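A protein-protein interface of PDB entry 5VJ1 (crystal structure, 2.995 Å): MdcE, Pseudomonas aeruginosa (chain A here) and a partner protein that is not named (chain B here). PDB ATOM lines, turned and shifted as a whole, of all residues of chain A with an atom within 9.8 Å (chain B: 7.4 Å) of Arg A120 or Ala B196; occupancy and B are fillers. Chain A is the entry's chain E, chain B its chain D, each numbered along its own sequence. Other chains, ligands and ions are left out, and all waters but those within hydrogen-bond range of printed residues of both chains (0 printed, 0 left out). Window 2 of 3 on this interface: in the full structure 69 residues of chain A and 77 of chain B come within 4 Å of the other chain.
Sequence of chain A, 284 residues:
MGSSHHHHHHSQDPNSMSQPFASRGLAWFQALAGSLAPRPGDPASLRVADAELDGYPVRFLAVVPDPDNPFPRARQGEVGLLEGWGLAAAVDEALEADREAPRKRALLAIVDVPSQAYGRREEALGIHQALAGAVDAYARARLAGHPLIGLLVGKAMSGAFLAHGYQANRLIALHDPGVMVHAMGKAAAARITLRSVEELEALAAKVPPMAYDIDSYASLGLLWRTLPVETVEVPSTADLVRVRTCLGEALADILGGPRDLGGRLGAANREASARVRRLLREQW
The side-chain carboxylate (OE2) of Glu B197 lies within hydrogen-bond range of the side-chain amide nitrogen (NE2) of Gln B268, 2.7 Å away.
O of Tyr A118 sits at hydrogen-bond distance from NE of Arg A73 (2.8 Å).
Of the 16 printed residues of chain B, 11 touch a printed residue of chain A.
Printed residues of chain B that touch a printed residue of chain A: Ile B189, Ala B193, Ala B196, Glu B197, Tyr B198, Phe B205, Leu B209, Thr B210, Gln B268, Pro B269 and Val B274.
Hydrophobic or aromatic side chains of chain B that line the printed part of chain A: Ile B189, Ala B193, Tyr B198, Phe B205, Leu B209, Pro B269 and Val B274.
Of the 16 printed residues of chain A, 7 touch a printed residue of chain B.
Printed residues of chain A that touch a printed residue of chain B: Arg A73, Tyr A118, Gly A119, Arg A120, Arg A121, Glu A123 and Ala A124.
Hydrophobic or aromatic side chains of chain A within 4 Å of the printed part of chain B: Ala A124.
Along chain A the printed residues that touch a printed residue of chain B span positions 73 to 124.
Among the printed residues, Asp or Glu carboxylates within 4 Å of a Lys or Arg side-chain nitrogen of the other chain: Arg A121 with Glu B197 (3.99 Å).
The backbone carbonyl oxygen of Ala B196 sits at hydrogen-bond distance from the guanidinium group of Arg A120 (2.9 Å).
OE1 of Glu B197 sits at hydrogen-bond distance from N of Arg A120 (2.6 Å).
The side-chain carboxylate (OE2) of Glu B197 is in salt-bridge range of the guanidinium group (NH2) of Arg A121 (3.99 Å).
The side-chain amide nitrogen (NE2) of Gln B268 lies close to the guanidinium group (NE) of Arg A120 (3.4 Å).
N of Gln B268 lies close to NH1 of Arg A121.
Among the printed residues, merely in contact across the chains: Arg A73 with Ala B193, Tyr A118 with Ala B193, Gly A119 with Ile B189, Gly A119 with Glu B197, Arg A120 with Tyr B198, Arg A120 with Phe B205, Arg A120 with Leu B209, Arg A121 with Pro B269, Glu A123 with Ile B189, Glu A123 with Thr B210 and Ala A124 with Val B274.
Of chain B, only Ala B196 (2.9 Å), Glu B197 (2.6 Å), Tyr B198 (3.6 Å), Phe B205 (3.6 Å), Leu B209 (3.6 Å) and Gln B268 (3.4 Å) come within 4 Å of Arg A120.
Of the printed residues of chain A, Ala B196 touches Arg A120 (2.9 Å).
Ile B195 touches none of the printed residues of chain A.
Of the printed residues of chain A, Phe B205 touches Arg A120 (3.6 Å).
Of the printed residues of chain A, Glu B197 touches Gly A119 (3.2 Å), Arg A120 (2.6 Å) and Arg A121 (3.99 Å).
Of the printed residues of chain B, Gly A119 touches Ile B189 and Glu B197.
Of the printed residues of chain A, Thr B210 touches Glu A123 (3.8 Å).
Of the printed residues of chain A, Ile B189 touches Gly A119 and Glu A123.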
ATOM      1  N   PHE A  71      10.411  20.620  12.108  1.00  0.00           N
ATOM      2  CA  PHE A  71       9.286  19.731  12.369  1.00  0.00           C
ATOM      3  C   PHE A  71       7.965  20.459  12.112  1.00  0.00           C
ATOM      4  O   PHE A  71       7.712  21.511  12.683  1.00  0.00           O
ATOM      5  CB  PHE A  71       9.358  19.206  13.802  1.00  0.00           C
ATOM      6  CG  PHE A  71      10.654  18.520  14.125  1.00  0.00           C
ATOM      7  CD1 PHE A  71      10.758  17.136  14.036  1.00  0.00           C
ATOM      8  CD2 PHE A  71      11.775  19.252  14.481  1.00  0.00           C
ATOM      9  CE1 PHE A  71      11.951  16.499  14.315  1.00  0.00           C
ATOM     10  CE2 PHE A  71      12.969  18.622  14.763  1.00  0.00           C
ATOM     11  CZ  PHE A  71      13.062  17.247  14.683  1.00  0.00           C
ATOM     12  N   PRO A  72       7.123  19.901  11.236  1.00  0.00           N
ATOM     13  CA  PRO A  72       5.869  20.543  10.830  1.00  0.00           C
ATOM     14  C   PRO A  72       4.904  20.676  11.992  1.00  0.00           C
ATOM     15  O   PRO A  72       4.198  21.682  12.088  1.00  0.00           O
ATOM     16  CB  PRO A  72       5.319  19.596   9.768  1.00  0.00           C
ATOM     17  CG  PRO A  72       6.517  18.852   9.281  1.00  0.00           C
ATOM     18  CD  PRO A  72       7.329  18.633  10.521  1.00  0.00           C
ATOM     19  N   ARG A  73       4.853  19.657  12.851  1.00  0.00           N
ATOM     20  CA  ARG A  73       3.949  19.658  14.009  1.00  0.00           C
ATOM     21  C   ARG A  73       4.372  20.611  15.157  1.00  0.00           C
ATOM     22  O   ARG A  73       3.898  20.482  16.290  1.00  0.00           O
ATOM     23  CB  ARG A  73       3.801  18.230  14.546  1.00  0.00           C
ATOM     24  CG  ARG A  73       3.204  17.248  13.555  1.00  0.00           C
ATOM     25  CD  ARG A  73       1.837  17.718  13.095  1.00  0.00           C
ATOM     26  NE  ARG A  73       0.992  18.105  14.221  1.00  0.00           N
ATOM     27  CZ  ARG A  73      -0.213  18.658  14.094  1.00  0.00           C
ATOM     28  NH1 ARG A  73      -0.719  18.877  12.887  1.00  0.00           N
ATOM     29  NH2 ARG A  73      -0.918  18.993  15.169  1.00  0.00           N
ATOM     30  N   ALA A  74       5.232  21.580  14.847  1.00  0.00           N
ATOM     31  CA  ALA A  74       5.745  22.523  15.827  1.00  0.00           C
ATOM     32  C   ALA A  74       5.912  23.896  15.187  1.00  0.00           C
ATOM     33  O   ALA A  74       6.885  24.618  15.471  1.00  0.00           O
ATOM     34  CB  ALA A  74       7.069  22.036  16.380  1.00  0.00           C
ATOM     35  N   LEU A  81      10.428  19.074  19.910  1.00  0.00           N
ATOM     36  CA  LEU A  81      11.775  18.542  20.110  1.00  0.00           C
ATOM     37  C   LEU A  81      12.877  19.582  20.242  1.00  0.00           C
ATOM     38  O   LEU A  81      13.690  19.528  21.173  1.00  0.00           O
ATOM     39  CB  LEU A  81      12.114  17.617  18.951  1.00  0.00           C
ATOM     40  CG  LEU A  81      11.368  16.297  18.971  1.00  0.00           C
ATOM     41  CD1 LEU A  81      11.469  15.653  17.614  1.00  0.00           C
ATOM     42  CD2 LEU A  81      12.030  15.414  20.031  1.00  0.00           C
ATOM     43  N   ALA A 117       4.189  19.793  21.186  1.00  0.00           N
ATOM     44  CA  ALA A 117       4.032  19.366  19.805  1.00  0.00           C
ATOM     45  C   ALA A 117       3.359  18.001  19.786  1.00  0.00           C
ATOM     46  O   ALA A 117       3.779  17.103  20.520  1.00  0.00           O
ATOM     47  CB  ALA A 117       5.374  19.326  19.093  1.00  0.00           C
ATOM     48  N   TYR A 118       2.318  17.865  18.956  1.00  0.00           N
ATOM     49  CA  TYR A 118       1.580  16.612  18.778  1.00  0.00           C
ATOM     50  C   TYR A 118       1.922  15.942  17.436  1.00  0.00           C
ATOM     51  O   TYR A 118       1.435  16.390  16.400  1.00  0.00           O
ATOM     52  CB  TYR A 118       0.067  16.874  18.810  1.00  0.00           C
ATOM     53  CG  TYR A 118      -0.552  17.314  20.124  1.00  0.00           C
ATOM     54  CD1 TYR A 118      -0.763  16.418  21.176  1.00  0.00           C
ATOM     55  CD2 TYR A 118      -0.986  18.616  20.287  1.00  0.00           C
ATOM     56  CE1 TYR A 118      -1.361  16.836  22.380  1.00  0.00           C
ATOM     57  CE2 TYR A 118      -1.579  19.043  21.472  1.00  0.00           C
ATOM     58  CZ  TYR A 118      -1.767  18.161  22.517  1.00  0.00           C
ATOM     59  OH  TYR A 118      -2.367  18.626  23.677  1.00  0.00           O
ATOM     60  N   GLY A 119       2.717  14.874  17.419  1.00  0.00           N
ATOM     61  CA  GLY A 119       3.042  14.259  16.134  1.00  0.00           C
ATOM     62  C   GLY A 119       3.912  13.010  16.132  1.00  0.00           C
ATOM     63  O   GLY A 119       4.552  12.722  17.133  1.00  0.00           O
ATOM     64  N   ARG A 120       3.932  12.268  15.018  1.00  0.00           N
ATOM     65  CA  ARG A 120       4.722  11.024  14.906  1.00  0.00           C
ATOM     66  C   ARG A 120       6.209  11.243  14.953  1.00  0.00           C
ATOM     67  O   ARG A 120       6.946  10.531  15.631  1.00  0.00           O
ATOM     68  CB  ARG A 120       4.416  10.281  13.607  1.00  0.00           C
ATOM     69  CG  ARG A 120       5.381   9.125  13.333  1.00  0.00           C
ATOM     70  CD  ARG A 120       5.206   8.551  11.926  1.00  0.00           C
ATOM     71  NE  ARG A 120       3.792   8.565  11.555  1.00  0.00           N
ATOM     72  CZ  ARG A 120       3.281   8.087  10.424  1.00  0.00           C
ATOM     73  NH1 ARG A 120       4.059   7.495   9.527  1.00  0.00           N
ATOM     74  NH2 ARG A 120       1.973   8.184  10.205  1.00  0.00           N
ATOM     75  N   ARG A 121       6.629  12.224  14.169  1.00  0.00           N
ATOM     76  CA  ARG A 121       8.008  12.652  14.090  1.00  0.00           C
ATOM     77  C   ARG A 121       8.479  12.905  15.516  1.00  0.00           C
ATOM     78  O   ARG A 121       9.507  12.377  15.945  1.00  0.00           O
ATOM     79  CB  ARG A 121       8.083  13.907  13.220  1.00  0.00           C
ATOM     80  CG  ARG A 121       9.266  14.039  12.292  1.00  0.00           C
ATOM     81  CD  ARG A 121       9.080  15.330  11.507  1.00  0.00           C
ATOM     82  NE  ARG A 121       7.773  15.394  10.837  1.00  0.00           N
ATOM     83  CZ  ARG A 121       7.498  14.826   9.665  1.00  0.00           C
ATOM     84  NH1 ARG A 121       8.455  14.184   9.013  1.00  0.00           N
ATOM     85  NH2 ARG A 121       6.284  14.930   9.131  1.00  0.00           N
ATOM     86  N   GLU A 122       7.643  13.628  16.265  1.00  0.00           N
ATOM     87  CA  GLU A 122       7.939  14.074  17.624  1.00  0.00           C
ATOM     88  C   GLU A 122       8.018  12.917  18.643  1.00  0.00           C
ATOM     89  O   GLU A 122       8.976  12.822  19.414  1.00  0.00           O
ATOM     90  CB  GLU A 122       6.894  15.114  18.047  1.00  0.00           C
ATOM     91  CG  GLU A 122       6.989  16.479  17.300  1.00  0.00           C
ATOM     92  CD  GLU A 122       6.515  16.461  15.830  1.00  0.00           C
ATOM     93  OE1 GLU A 122       6.747  17.473  15.118  1.00  0.00           O
ATOM     94  OE2 GLU A 122       5.902  15.460  15.378  1.00  0.00           O
ATOM     95  N   GLU A 123       7.031  12.028  18.629  1.00  0.00           N
ATOM     96  CA  GLU A 123       7.006  10.866  19.526  1.00  0.00           C
ATOM     97  C   GLU A 123       8.110   9.854  19.215  1.00  0.00           C
ATOM     98  O   GLU A 123       8.620   9.162  20.109  1.00  0.00           O
ATOM     99  CB  GLU A 123       5.658  10.156  19.432  1.00  0.00           C
ATOM    100  CG  GLU A 123       4.519  10.863  20.139  1.00  0.00           C
ATOM    101  CD  GLU A 123       4.693  10.940  21.637  1.00  0.00           C
ATOM    102  OE1 GLU A 123       5.033   9.901  22.240  1.00  0.00           O
ATOM    103  OE2 GLU A 123       4.464  12.034  22.202  1.00  0.00           O
ATOM    104  N   ALA A 124       8.454   9.747  17.934  1.00  0.00           N
ATOM    105  CA  ALA A 124       9.450   8.777  17.498  1.00  0.00           C
ATOM    106  C   ALA A 124      10.817   9.168  18.026  1.00  0.00           C
ATOM    107  O   ALA A 124      11.621   8.308  18.380  1.00  0.00           O
ATOM    108  CB  ALA A 124       9.474   8.674  15.972  1.00  0.00           C
ATOM    109  N   LEU A 125      11.057  10.473  18.110  1.00  0.00           N
ATOM    110  CA  LEU A 125      12.378  10.971  18.456  1.00  0.00           C
ATOM    111  C   LEU A 125      12.533  11.284  19.944  1.00  0.00           C
ATOM    112  O   LEU A 125      13.582  11.775  20.374  1.00  0.00           O
ATOM    113  CB  LEU A 125      12.698  12.204  17.612  1.00  0.00           C
ATOM    114  CG  LEU A 125      12.880  11.858  16.130  1.00  0.00           C
ATOM    115  CD1 LEU A 125      12.786  13.105  15.286  1.00  0.00           C
ATOM    116  CD2 LEU A 125      14.191  11.133  15.877  1.00  0.00           C
ATOM    117  N   GLY A 126      11.487  11.006  20.718  1.00  0.00           N
ATOM    118  CA  GLY A 126      11.534  11.145  22.165  1.00  0.00           C
ATOM    119  C   GLY A 126      11.240  12.533  22.697  1.00  0.00           C
ATOM    120  O   GLY A 126      11.979  13.025  23.556  1.00  0.00           O
ATOM    121  N   ILE A 127      10.147  13.141  22.235  1.00  0.00           N
ATOM    122  CA  ILE A 127       9.782  14.491  22.667  1.00  0.00           C
ATOM    123  C   ILE A 127       9.583  14.572  24.186  1.00  0.00           C
ATOM    124  O   ILE A 127       9.790  15.624  24.793  1.00  0.00           O
ATOM    125  CB  ILE A 127       8.507  15.002  21.935  1.00  0.00           C
ATOM    126  CG1 ILE A 127       8.198  16.462  22.296  1.00  0.00           C
ATOM    127  CG2 ILE A 127       7.322  14.116  22.219  1.00  0.00           C
ATOM    128  CD1 ILE A 127       7.052  17.074  21.489  1.00  0.00           C
ATOM    129  N   ILE B 189      -2.892  12.302  19.748  1.00  0.00           N
ATOM    130  CA  ILE B 189      -2.163  12.773  18.575  1.00  0.00           C
ATOM    131  C   ILE B 189      -3.039  12.657  17.343  1.00  0.00           C
ATOM    132  O   ILE B 189      -3.145  13.592  16.566  1.00  0.00           O
ATOM    133  CB  ILE B 189      -0.880  11.992  18.340  1.00  0.00           C
ATOM    134  CG1 ILE B 189       0.084  12.185  19.498  1.00  0.00           C
ATOM    135  CG2 ILE B 189      -0.211  12.483  17.110  1.00  0.00           C
ATOM    136  CD1 ILE B 189       1.296  11.329  19.384  1.00  0.00           C
ATOM    137  N   GLU B 190      -3.672  11.501  17.175  1.00  0.00           N
ATOM    138  CA  GLU B 190      -4.601  11.282  16.071  1.00  0.00           C
ATOM    139  C   GLU B 190      -5.618  12.400  16.073  1.00  0.00           C
ATOM    140  O   GLU B 190      -5.941  12.975  15.032  1.00  0.00           O
ATOM    141  CB  GLU B 190      -5.308   9.936  16.205  1.00  0.00           C
ATOM    142  CG  GLU B 190      -6.357   9.684  15.144  1.00  0.00           C
ATOM    143  CD  GLU B 190      -7.050   8.333  15.307  1.00  0.00           C
ATOM    144  OE1 GLU B 190      -6.356   7.295  15.451  1.00  0.00           O
ATOM    145  OE2 GLU B 190      -8.301   8.316  15.291  1.00  0.00           O
ATOM    146  N   ALA B 193      -3.641  15.885  15.397  1.00  0.00           N
ATOM    147  CA  ALA B 193      -2.810  15.906  14.180  1.00  0.00           C
ATOM    148  C   ALA B 193      -3.361  15.164  12.955  1.00  0.00           C
ATOM    149  O   ALA B 193      -2.781  15.257  11.865  1.00  0.00           O
ATOM    150  CB  ALA B 193      -1.409  15.361  14.499  1.00  0.00           C
ATOM    151  N   GLY B 194      -4.435  14.400  13.127  1.00  0.00           N
ATOM    152  CA  GLY B 194      -5.023  13.692  12.005  1.00  0.00           C
ATOM    153  C   GLY B 194      -4.655  12.219  11.966  1.00  0.00           C
ATOM    154  O   GLY B 194      -3.534  11.838  12.330  1.00  0.00           O
ATOM    155  N   ILE B 195      -5.601  11.393  11.516  1.00  0.00           N
ATOM    156  CA  ILE B 195      -5.427   9.939  11.456  1.00  0.00           C
ATOM    157  C   ILE B 195      -4.250   9.484  10.573  1.00  0.00           C
ATOM    158  O   ILE B 195      -3.699   8.395  10.754  1.00  0.00           O
ATOM    159  CB  ILE B 195      -6.725   9.279  10.953  1.00  0.00           C
ATOM    160  CG1 ILE B 195      -6.611   7.756  11.024  1.00  0.00           C
ATOM    161  CG2 ILE B 195      -7.036   9.728   9.533  1.00  0.00           C
ATOM    162  CD1 ILE B 195      -7.929   7.036  10.850  1.00  0.00           C
ATOM    163  N   ALA B 196      -3.846  10.341   9.645  1.00  0.00           N
ATOM    164  CA  ALA B 196      -2.720  10.070   8.763  1.00  0.00           C
ATOM    165  C   ALA B 196      -1.390  10.242   9.493  1.00  0.00           C
ATOM    166  O   ALA B 196      -0.439   9.496   9.246  1.00  0.00           O
ATOM    167  CB  ALA B 196      -2.781  10.970   7.552  1.00  0.00           C
ATOM    168  N   GLU B 197      -1.305  11.272  10.337  1.00  0.00           N
ATOM    169  CA  GLU B 197      -0.080  11.562  11.094  1.00  0.00           C
ATOM    170  C   GLU B 197       0.210  10.532  12.191  1.00  0.00           C
ATOM    171  O   GLU B 197       1.358  10.344  12.562  1.00  0.00           O
ATOM    172  CB  GLU B 197      -0.141  12.979  11.704  1.00  0.00           C
ATOM    173  CG  GLU B 197       1.073  13.895  11.361  1.00  0.00           C
ATOM    174  CD  GLU B 197       2.321  13.536  12.158  1.00  0.00           C
ATOM    175  OE1 GLU B 197       2.168  13.111  13.320  1.00  0.00           O
ATOM    176  OE2 GLU B 197       3.449  13.652  11.628  1.00  0.00           O
ATOM    177  N   TYR B 198      -0.823   9.869  12.699  1.00  0.00           N
ATOM    178  CA  TYR B 198      -0.674   8.869  13.768  1.00  0.00           C
ATOM    179  C   TYR B 198      -1.987   8.091  13.900  1.00  0.00           C
ATOM    180  O   TYR B 198      -3.059   8.693  13.969  1.00  0.00           O
ATOM    181  CB  TYR B 198      -0.289   9.553  15.092  1.00  0.00           C
ATOM    182  CG  TYR B 198       0.609   8.780  16.045  1.00  0.00           C
ATOM    183  CD1 TYR B 198       1.974   9.048  16.135  1.00  0.00           C
ATOM    184  CD2 TYR B 198       0.087   7.801  16.885  1.00  0.00           C
ATOM    185  CE1 TYR B 198       2.802   8.344  17.033  1.00  0.00           C
ATOM    186  CE2 TYR B 198       0.899   7.100  17.781  1.00  0.00           C
ATOM    187  CZ  TYR B 198       2.248   7.374  17.850  1.00  0.00           C
ATOM    188  OH  TYR B 198       3.028   6.669  18.739  1.00  0.00           O
ATOM    189  N   ASP B 199      -1.904   6.765  13.964  1.00  0.00           N
ATOM    190  CA  ASP B 199      -3.097   5.909  13.978  1.00  0.00           C
ATOM    191  C   ASP B 199      -3.328   5.237  15.328  1.00  0.00           C
ATOM    192  O   ASP B 199      -2.574   4.336  15.699  1.00  0.00           O
ATOM    193  CB  ASP B 199      -2.958   4.824  12.916  1.00  0.00           C
ATOM    194  CG  ASP B 199      -4.258   4.127  12.620  1.00  0.00           C
ATOM    195  OD1 ASP B 199      -5.069   3.950  13.552  1.00  0.00           O
ATOM    196  OD2 ASP B 199      -4.444   3.702  11.458  1.00  0.00           O
ATOM    197  N   PHE B 205       2.309  -0.491  15.208  1.00  0.00           N
ATOM    198  CA  PHE B 205       2.949   0.788  14.880  1.00  0.00           C
ATOM    199  C   PHE B 205       3.249   1.597  16.150  1.00  0.00           C
ATOM    200  O   PHE B 205       4.341   2.161  16.308  1.00  0.00           O
ATOM    201  CB  PHE B 205       2.038   1.572  13.925  1.00  0.00           C
ATOM    202  CG  PHE B 205       2.313   3.051  13.844  1.00  0.00           C
ATOM    203  CD1 PHE B 205       3.426   3.538  13.184  1.00  0.00           C
ATOM    204  CD2 PHE B 205       1.420   3.966  14.393  1.00  0.00           C
ATOM    205  CE1 PHE B 205       3.656   4.931  13.090  1.00  0.00           C
ATOM    206  CE2 PHE B 205       1.643   5.352  14.302  1.00  0.00           C
ATOM    207  CZ  PHE B 205       2.759   5.830  13.651  1.00  0.00           C
ATOM    208  N   LEU B 209       7.287   2.621  17.673  1.00  0.00           N
ATOM    209  CA  LEU B 209       7.919   3.913  17.933  1.00  0.00           C
ATOM    210  C   LEU B 209       8.086   4.211  19.417  1.00  0.00           C
ATOM    211  O   LEU B 209       9.101   4.783  19.821  1.00  0.00           O
ATOM    212  CB  LEU B 209       7.123   5.043  17.283  1.00  0.00           C
ATOM    213  CG  LEU B 209       6.922   4.922  15.779  1.00  0.00           C
ATOM    214  CD1 LEU B 209       6.307   6.187  15.243  1.00  0.00           C
ATOM    215  CD2 LEU B 209       8.251   4.642  15.112  1.00  0.00           C
ATOM    216  N   THR B 210       7.109   3.817  20.232  1.00  0.00           N
ATOM    217  CA  THR B 210       7.126   4.182  21.650  1.00  0.00           C
ATOM    218  C   THR B 210       7.208   2.973  22.582  1.00  0.00           C
ATOM    219  O   THR B 210       7.113   3.114  23.810  1.00  0.00           O
ATOM    220  CB  THR B 210       5.871   5.034  22.040  1.00  0.00           C
ATOM    221  OG1 THR B 210       4.689   4.239  21.911  1.00  0.00           O
ATOM    222  CG2 THR B 210       5.732   6.286  21.141  1.00  0.00           C
ATOM    223  N   GLN B 268       8.779  11.220   7.278  1.00  0.00           N
ATOM    224  CA  GLN B 268       8.407  10.519   8.525  1.00  0.00           C
ATOM    225  C   GLN B 268       9.413   9.462   8.976  1.00  0.00           C
ATOM    226  O   GLN B 268       9.495   8.393   8.369  1.00  0.00           O
ATOM    227  CB  GLN B 268       7.023   9.876   8.368  1.00  0.00           C
ATOM    228  CG  GLN B 268       5.875  10.854   8.417  1.00  0.00           C
ATOM    229  CD  GLN B 268       5.563  11.330   9.834  1.00  0.00           C
ATOM    230  OE1 GLN B 268       6.469  11.542  10.637  1.00  0.00           O
ATOM    231  NE2 GLN B 268       4.278  11.560  10.123  1.00  0.00           N
ATOM    232  N   PRO B 269      10.165   9.749  10.053  1.00  0.00           N
ATOM    233  CA  PRO B 269      11.134   8.754  10.515  1.00  0.00           C
ATOM    234  C   PRO B 269      10.423   7.471  10.903  1.00  0.00           C
ATOM    235  O   PRO B 269       9.254   7.536  11.272  1.00  0.00           O
ATOM    236  CB  PRO B 269      11.779   9.436  11.727  1.00  0.00           C
ATOM    237  CG  PRO B 269      10.704  10.333  12.226  1.00  0.00           C
ATOM    238  CD  PRO B 269      10.092  10.892  10.975  1.00  0.00           C
ATOM    239  N   ASP B 270      11.109   6.335  10.825  1.00  0.00           N
ATOM    240  CA  ASP B 270      10.497   5.069  11.204  1.00  0.00           C
ATOM    241  C   ASP B 270      11.291   4.486  12.365  1.00  0.00           C
ATOM    242  O   ASP B 270      12.364   4.992  12.683  1.00  0.00           O
ATOM    243  CB  ASP B 270      10.426   4.092  10.012  1.00  0.00           C
ATOM    244  CG  ASP B 270      11.796   3.735   9.442  1.00  0.00           C
ATOM    245  OD1 ASP B 270      12.538   2.966  10.097  1.00  0.00           O
ATOM    246  OD2 ASP B 270      12.122   4.203   8.326  1.00  0.00           O
ATOM    247  N   VAL B 274      15.167   5.912  13.658  1.00  0.00           N
ATOM    248  CA  VAL B 274      15.438   6.522  14.950  1.00  0.00           C
ATOM    249  C   VAL B 274      16.603   5.848  15.678  1.00  0.00           C
ATOM    250  O   VAL B 274      17.343   6.518  16.398  1.00  0.00           O
ATOM    251  CB  VAL B 274      14.163   6.489  15.849  1.00  0.00           C
ATOM    252  CG1 VAL B 274      14.462   6.950  17.273  1.00  0.00           C
ATOM    253  CG2 VAL B 274      13.052   7.339  15.236  1.00  0.00           C
